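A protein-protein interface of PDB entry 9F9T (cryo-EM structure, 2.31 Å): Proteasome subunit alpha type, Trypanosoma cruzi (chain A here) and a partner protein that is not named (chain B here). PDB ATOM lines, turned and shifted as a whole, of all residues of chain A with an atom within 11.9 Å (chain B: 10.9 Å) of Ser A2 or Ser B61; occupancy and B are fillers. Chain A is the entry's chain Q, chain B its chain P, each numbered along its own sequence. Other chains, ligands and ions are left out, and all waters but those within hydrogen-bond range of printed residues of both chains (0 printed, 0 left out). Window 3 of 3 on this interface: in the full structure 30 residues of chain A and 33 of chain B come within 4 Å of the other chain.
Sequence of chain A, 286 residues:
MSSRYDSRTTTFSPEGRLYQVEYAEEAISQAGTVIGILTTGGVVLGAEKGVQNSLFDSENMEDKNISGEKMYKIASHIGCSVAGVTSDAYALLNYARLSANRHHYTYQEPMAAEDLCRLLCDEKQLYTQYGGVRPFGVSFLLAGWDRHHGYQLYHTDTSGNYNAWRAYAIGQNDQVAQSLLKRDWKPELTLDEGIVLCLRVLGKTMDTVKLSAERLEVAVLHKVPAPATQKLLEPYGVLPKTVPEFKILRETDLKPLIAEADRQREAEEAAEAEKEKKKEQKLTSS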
ATOM      1  N   SER A   2      -1.053  17.905  18.752  1.00  0.00           N
ATOM      2  CA  SER A   2      -0.209  18.503  19.825  1.00  0.00           C
ATOM      3  C   SER A   2      -0.922  19.712  20.461  1.00  0.00           C
ATOM      4  O   SER A   2      -0.677  19.993  21.642  1.00  0.00           O
ATOM      5  CB  SER A   2       1.207  18.876  19.329  1.00  0.00           C
ATOM      6  OG  SER A   2       2.246  18.462  20.219  1.00  0.00           O
ATOM      7  N   SER A   3      -1.788  20.429  19.713  1.00  0.00           N
ATOM      8  CA  SER A   3      -2.508  21.577  20.264  1.00  0.00           C
ATOM      9  C   SER A   3      -3.468  21.194  21.403  1.00  0.00           C
ATOM     10  O   SER A   3      -3.774  22.054  22.219  1.00  0.00           O
ATOM     11  CB  SER A   3      -3.247  22.368  19.195  1.00  0.00           C
ATOM     12  OG  SER A   3      -4.343  21.633  18.665  1.00  0.00           O
ATOM     13  N   ARG A   4      -3.891  19.921  21.500  1.00  0.00           N
ATOM     14  CA  ARG A   4      -4.720  19.450  22.604  1.00  0.00           C
ATOM     15  C   ARG A   4      -3.940  19.312  23.917  1.00  0.00           C
ATOM     16  O   ARG A   4      -4.559  19.210  24.972  1.00  0.00           O
ATOM     17  CB  ARG A   4      -5.459  18.148  22.243  1.00  0.00           C
ATOM     18  CG  ARG A   4      -4.595  16.904  22.134  1.00  0.00           C
ATOM     19  CD  ARG A   4      -5.255  15.751  21.386  1.00  0.00           C
ATOM     20  NE  ARG A   4      -6.172  14.981  22.221  1.00  0.00           N
ATOM     21  CZ  ARG A   4      -7.369  14.539  21.838  1.00  0.00           C
ATOM     22  NH1 ARG A   4      -8.119  13.861  22.689  1.00  0.00           N
ATOM     23  NH2 ARG A   4      -7.813  14.769  20.611  1.00  0.00           N
ATOM     24  N   TYR A   5      -2.599  19.315  23.865  1.00  0.00           N
ATOM     25  CA  TYR A   5      -1.738  19.182  25.041  1.00  0.00           C
ATOM     26  C   TYR A   5      -1.178  20.548  25.451  1.00  0.00           C
ATOM     27  O   TYR A   5      -0.316  20.608  26.325  1.00  0.00           O
ATOM     28  CB  TYR A   5      -0.616  18.160  24.759  1.00  0.00           C
ATOM     29  CG  TYR A   5      -1.070  16.786  24.238  1.00  0.00           C
ATOM     30  CD1 TYR A   5      -1.946  15.980  24.964  1.00  0.00           C
ATOM     31  CD2 TYR A   5      -0.683  16.329  22.963  1.00  0.00           C
ATOM     32  CE1 TYR A   5      -2.372  14.746  24.476  1.00  0.00           C
ATOM     33  CE2 TYR A   5      -1.125  15.115  22.450  1.00  0.00           C
ATOM     34  CZ  TYR A   5      -1.958  14.310  23.218  1.00  0.00           C
ATOM     35  OH  TYR A   5      -2.373  13.117  22.703  1.00  0.00           O
ATOM     36  N   ASP A   6      -1.626  21.625  24.770  1.00  0.00           N
ATOM     37  CA  ASP A   6      -1.290  23.012  25.085  1.00  0.00           C
ATOM     38  C   ASP A   6      -2.010  23.358  26.381  1.00  0.00           C
ATOM     39  O   ASP A   6      -3.149  22.944  26.570  1.00  0.00           O
ATOM     40  CB  ASP A   6      -1.648  23.966  23.923  1.00  0.00           C
ATOM     41  CG  ASP A   6      -1.213  25.423  24.038  1.00  0.00           C
ATOM     42  OD1 ASP A   6      -0.784  25.801  25.122  1.00  0.00           O
ATOM     43  OD2 ASP A   6      -1.295  26.183  23.019  1.00  0.00           O
ATOM     44  N   SER A   7      -1.284  24.044  27.271  1.00  0.00           N
ATOM     45  CA  SER A   7      -1.696  24.412  28.623  1.00  0.00           C
ATOM     46  C   SER A   7      -2.413  25.770  28.653  1.00  0.00           C
ATOM     47  O   SER A   7      -3.231  26.036  29.529  1.00  0.00           O
ATOM     48  CB  SER A   7      -0.452  24.436  29.495  1.00  0.00           C
ATOM     49  OG  SER A   7       0.658  25.044  28.799  1.00  0.00           O
ATOM     50  N   ARG A   8      -2.024  26.648  27.714  1.00  0.00           N
ATOM     51  CA  ARG A   8      -2.735  27.870  27.387  1.00  0.00           C
ATOM     52  C   ARG A   8      -2.391  28.921  28.452  1.00  0.00           C
ATOM     53  O   ARG A   8      -3.264  29.541  29.077  1.00  0.00           O
ATOM     54  CB  ARG A   8      -4.224  27.567  27.148  1.00  0.00           C
ATOM     55  CG  ARG A   8      -4.488  26.756  25.878  1.00  0.00           C
ATOM     56  CD  ARG A   8      -5.950  26.465  25.556  1.00  0.00           C
ATOM     57  NE  ARG A   8      -6.101  25.616  24.371  1.00  0.00           N
ATOM     58  CZ  ARG A   8      -5.941  26.012  23.102  1.00  0.00           C
ATOM     59  NH1 ARG A   8      -5.920  25.113  22.128  1.00  0.00           N
ATOM     60  NH2 ARG A   8      -5.770  27.295  22.808  1.00  0.00           N
ATOM     61  N   THR A   9      -1.074  29.156  28.575  1.00  0.00           N
ATOM     62  CA  THR A   9      -0.476  29.898  29.679  1.00  0.00           C
ATOM     63  C   THR A   9      -0.903  31.363  29.632  1.00  0.00           C
ATOM     64  O   THR A   9      -0.889  32.026  30.666  1.00  0.00           O
ATOM     65  CB  THR A   9       1.070  29.785  29.700  1.00  0.00           C
ATOM     66  OG1 THR A   9       1.622  30.237  28.452  1.00  0.00           O
ATOM     67  CG2 THR A   9       1.548  28.387  30.049  1.00  0.00           C
ATOM     68  N   GLY A 131       3.293  34.395  23.858  1.00  0.00           N
ATOM     69  CA  GLY A 131       4.408  33.457  23.706  1.00  0.00           C
ATOM     70  C   GLY A 131       4.210  32.021  24.238  1.00  0.00           C
ATOM     71  O   GLY A 131       5.159  31.236  24.214  1.00  0.00           O
ATOM     72  N   GLY A 132       3.010  31.646  24.723  1.00  0.00           N
ATOM     73  CA  GLY A 132       2.748  30.244  25.053  1.00  0.00           C
ATOM     74  C   GLY A 132       3.662  29.570  26.103  1.00  0.00           C
ATOM     75  O   GLY A 132       3.571  28.367  26.309  1.00  0.00           O
ATOM     76  N   VAL A 133       4.472  30.321  26.854  1.00  0.00           N
ATOM     77  CA  VAL A 133       5.324  29.735  27.890  1.00  0.00           C
ATOM     78  C   VAL A 133       4.982  30.309  29.270  1.00  0.00           C
ATOM     79  O   VAL A 133       4.407  31.401  29.361  1.00  0.00           O
ATOM     80  CB  VAL A 133       6.818  29.957  27.559  1.00  0.00           C
ATOM     81  CG1 VAL A 133       7.270  29.179  26.313  1.00  0.00           C
ATOM     82  CG2 VAL A 133       7.184  31.450  27.456  1.00  0.00           C
ATOM     83  N   SER B  61       5.816  22.386  17.590  1.00  0.00           N
ATOM     84  CA  SER B  61       5.024  22.654  18.827  1.00  0.00           C
ATOM     85  C   SER B  61       5.797  23.638  19.718  1.00  0.00           C
ATOM     86  O   SER B  61       6.848  23.291  20.242  1.00  0.00           O
ATOM     87  CB  SER B  61       4.644  21.349  19.564  1.00  0.00           C
ATOM     88  OG  SER B  61       3.378  20.823  19.145  1.00  0.00           O
ATOM     89  N   ALA B  62       5.286  24.875  19.860  1.00  0.00           N
ATOM     90  CA  ALA B  62       6.022  25.967  20.480  1.00  0.00           C
ATOM     91  C   ALA B  62       5.333  26.442  21.779  1.00  0.00           C
ATOM     92  O   ALA B  62       5.496  27.592  22.217  1.00  0.00           O
ATOM     93  CB  ALA B  62       6.151  27.082  19.470  1.00  0.00           C
ATOM     94  N   TYR B  63       4.611  25.537  22.457  1.00  0.00           N
ATOM     95  CA  TYR B  63       4.057  25.901  23.751  1.00  0.00           C
ATOM     96  C   TYR B  63       4.876  25.294  24.887  1.00  0.00           C
ATOM     97  O   TYR B  63       5.476  24.245  24.716  1.00  0.00           O
ATOM     98  CB  TYR B  63       2.576  25.530  23.834  1.00  0.00           C
ATOM     99  CG  TYR B  63       2.274  24.062  23.660  1.00  0.00           C
ATOM    100  CD1 TYR B  63       2.378  23.172  24.714  1.00  0.00           C
ATOM    101  CD2 TYR B  63       1.876  23.583  22.421  1.00  0.00           C
ATOM    102  CE1 TYR B  63       2.089  21.825  24.528  1.00  0.00           C
ATOM    103  CE2 TYR B  63       1.573  22.244  22.226  1.00  0.00           C
ATOM    104  CZ  TYR B  63       1.699  21.361  23.277  1.00  0.00           C
ATOM    105  OH  TYR B  63       1.359  20.071  23.039  1.00  0.00           O
ATOM    106  N   GLY B  64       4.894  25.952  26.052  1.00  0.00           N
ATOM    107  CA  GLY B  64       5.643  25.423  27.179  1.00  0.00           C
ATOM    108  C   GLY B  64       5.075  24.129  27.743  1.00  0.00           C
ATOM    109  O   GLY B  64       3.860  23.968  27.845  1.00  0.00           O
ATOM    110  N   LEU B  65       5.962  23.219  28.155  1.00  0.00           N
ATOM    111  CA  LEU B  65       5.572  21.922  28.714  1.00  0.00           C
ATOM    112  C   LEU B  65       5.683  21.943  30.244  1.00  0.00           C
ATOM    113  O   LEU B  65       5.088  21.106  30.941  1.00  0.00           O
ATOM    114  CB  LEU B  65       6.455  20.832  28.073  1.00  0.00           C
ATOM    115  CG  LEU B  65       6.291  20.672  26.546  1.00  0.00           C
ATOM    116  CD1 LEU B  65       7.272  19.646  25.970  1.00  0.00           C
ATOM    117  CD2 LEU B  65       4.847  20.304  26.180  1.00  0.00           C
ATOM    118  N   THR B  66       6.423  22.935  30.737  1.00  0.00           N
ATOM    119  CA  THR B  66       6.714  23.130  32.149  1.00  0.00           C
ATOM    120  C   THR B  66       5.933  24.344  32.630  1.00  0.00           C
ATOM    121  O   THR B  66       6.144  25.421  32.065  1.00  0.00           O
ATOM    122  CB  THR B  66       8.226  23.369  32.385  1.00  0.00           C
ATOM    123  OG1 THR B  66       8.996  22.283  31.850  1.00  0.00           O
ATOM    124  CG2 THR B  66       8.559  23.583  33.850  1.00  0.00           C
ATOM    125  N   GLN B 178      11.518  26.762  30.479  1.00  0.00           N
ATOM    126  CA  GLN B 178      10.657  27.884  30.140  1.00  0.00           C
ATOM    127  C   GLN B 178      10.295  27.919  28.652  1.00  0.00           C
ATOM    128  O   GLN B 178       9.143  28.151  28.318  1.00  0.00           O
ATOM    129  CB  GLN B 178      11.293  29.206  30.555  1.00  0.00           C
ATOM    130  CG  GLN B 178      10.248  30.208  31.031  1.00  0.00           C
ATOM    131  CD  GLN B 178      10.788  31.598  31.222  1.00  0.00           C
ATOM    132  OE1 GLN B 178      11.869  31.946  30.751  1.00  0.00           O
ATOM    133  NE2 GLN B 178      10.008  32.427  31.894  1.00  0.00           N
ATOM    134  N   SER B 179      11.275  27.726  27.772  1.00  0.00           N
ATOM    135  CA  SER B 179      11.121  27.447  26.336  1.00  0.00           C
ATOM    136  C   SER B 179       9.938  26.537  25.978  1.00  0.00           C
ATOM    137  O   SER B 179       9.526  25.645  26.740  1.00  0.00           O
ATOM    138  CB  SER B 179      12.429  26.865  25.760  1.00  0.00           C
ATOM    139  OG  SER B 179      13.454  27.864  25.683  1.00  0.00           O
ATOM    140  N   GLY B 180       9.386  26.814  24.789  1.00  0.00           N
ATOM    141  CA  GLY B 180       8.254  26.069  24.264  1.00  0.00           C
ATOM    142  C   GLY B 180       8.634  24.765  23.539  1.00  0.00           C
ATOM    143  O   GLY B 180       9.631  24.691  22.819  1.00  0.00           O
ATOM    144  N   GLY B 181       7.847  23.717  23.832  1.00  0.00           N
ATOM    145  CA  GLY B 181       8.027  22.397  23.251  1.00  0.00           C
ATOM    146  C   GLY B 181       9.221  21.571  23.762  1.00  0.00           C
ATOM    147  O   GLY B 181       9.583  20.586  23.099  1.00  0.00           O
ATOM    148  N   VAL B 182       9.758  21.870  24.969  1.00  0.00           N
ATOM    149  CA  VAL B 182      10.891  21.100  25.470  1.00  0.00           C
ATOM    150  C   VAL B 182      10.645  20.590  26.866  1.00  0.00           C
ATOM    151  O   VAL B 182      10.070  21.312  27.665  1.00  0.00           O
ATOM    152  CB  VAL B 182      12.209  21.900  25.396  1.00  0.00           C
ATOM    153  CG1 VAL B 182      12.551  22.256  23.966  1.00  0.00           C
ATOM    154  CG2 VAL B 182      12.176  23.159  26.219  1.00  0.00           C
ATOM    155  N   ARG B 183      11.173  19.409  27.183  1.00  0.00           N
ATOM    156  CA  ARG B 183      11.263  19.001  28.551  1.00  0.00           C
ATOM    157  C   ARG B 183      12.597  19.386  29.168  1.00  0.00           C
ATOM    158  O   ARG B 183      13.560  19.694  28.486  1.00  0.00           O
ATOM    159  CB  ARG B 183      11.117  17.506  28.764  1.00  0.00           C
ATOM    160  CG  ARG B 183      12.192  16.665  28.117  1.00  0.00           C
ATOM    161  CD  ARG B 183      12.201  15.300  28.730  1.00  0.00           C
ATOM    162  NE  ARG B 183      13.173  14.534  27.964  1.00  0.00           N
ATOM    163  CZ  ARG B 183      14.480  14.629  28.113  1.00  0.00           C
ATOM    164  NH1 ARG B 183      15.278  13.926  27.343  1.00  0.00           N
ATOM    165  NH2 ARG B 183      15.009  15.389  29.064  1.00  0.00           N
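The backbone carbonyl oxygen of Tyr B63 lies within hydrogen-bond range of the backbone NH of Gly B181 (2.6 Å).
N of Arg A8 is in hydrogen-bond range of OD1 of Asp A6.
The side-chain hydroxyl of Thr A9 sits close to the backbone carbonyl oxygen of Gly A132 (3.4 Å).
O of Val A133 lies within hydrogen-bond range of OG1 of Thr A9 (3.2 Å).
Hydrophobic or aromatic side chains of chain B within 4 Å of the printed part of chain A: Tyr B63.
Among the printed residues, 10 pairs touch across the chains.
Of chain B, only Ser B61 and Tyr B63 come within 4 Å of Ser A2.
No residue of chain B comes within 4 Å of Ser A3.
Asp A6 touches just one residue of chain B: Tyr B63 (3.6 Å).
Of the printed residues of chain B, Ser A7 touches Gly B64.
Of chain A, only Ser A2 (2.8 Å) comes within 4 Å of Ser B61.
Tyr B63 touches just these residues of chain A: Ser A2 (2.5 Å), Tyr A5 (3.2 Å), Asp A6 (3.6 Å) and Gly A132 (3.6 Å).
Of the printed residues of chain A, Gly B64 touches Ser A7 and Gly A132.
Leu B65 touches none of the printed residues of chain A.
Of the printed residues of chain A, Ser B179 touches Val A133.
Gly B180 touches just one residue of chain A: Val A133 (3.5 Å).
Gly B181 touches none of the printed residues of chain A.
The nearest residue of chain B that does not touch Ser A2 is Leu B65 (6.8 Å).
The nearest residue of chain A that does not touch Ser B61 is Ser A3 (5.2 Å).
The nearest printed residue of chain A that does not touch Gly B64 is Val A133 (4.02 Å).
The side-chain hydroxyl (OG) of Ser B61 is in hydrogen-bond range of the side-chain hydroxyl (OG) of Ser A2.
OH of Tyr B63 is in hydrogen-bond range of O of Ser A2, 2.5 Å away.
N of Gly B64 lies within hydrogen-bond range of O of Gly A132, at 2.8 Å.
Among the printed residues, pairs that only touch across the chains: Tyr A5 with Tyr B63, Asp A6 with Tyr B63, Ser A7 with Gly B64, Gly A132 with Tyr B63, Val A133 with Gln B178, Val A133 with Ser B179 and Val A133 with Gly B180.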
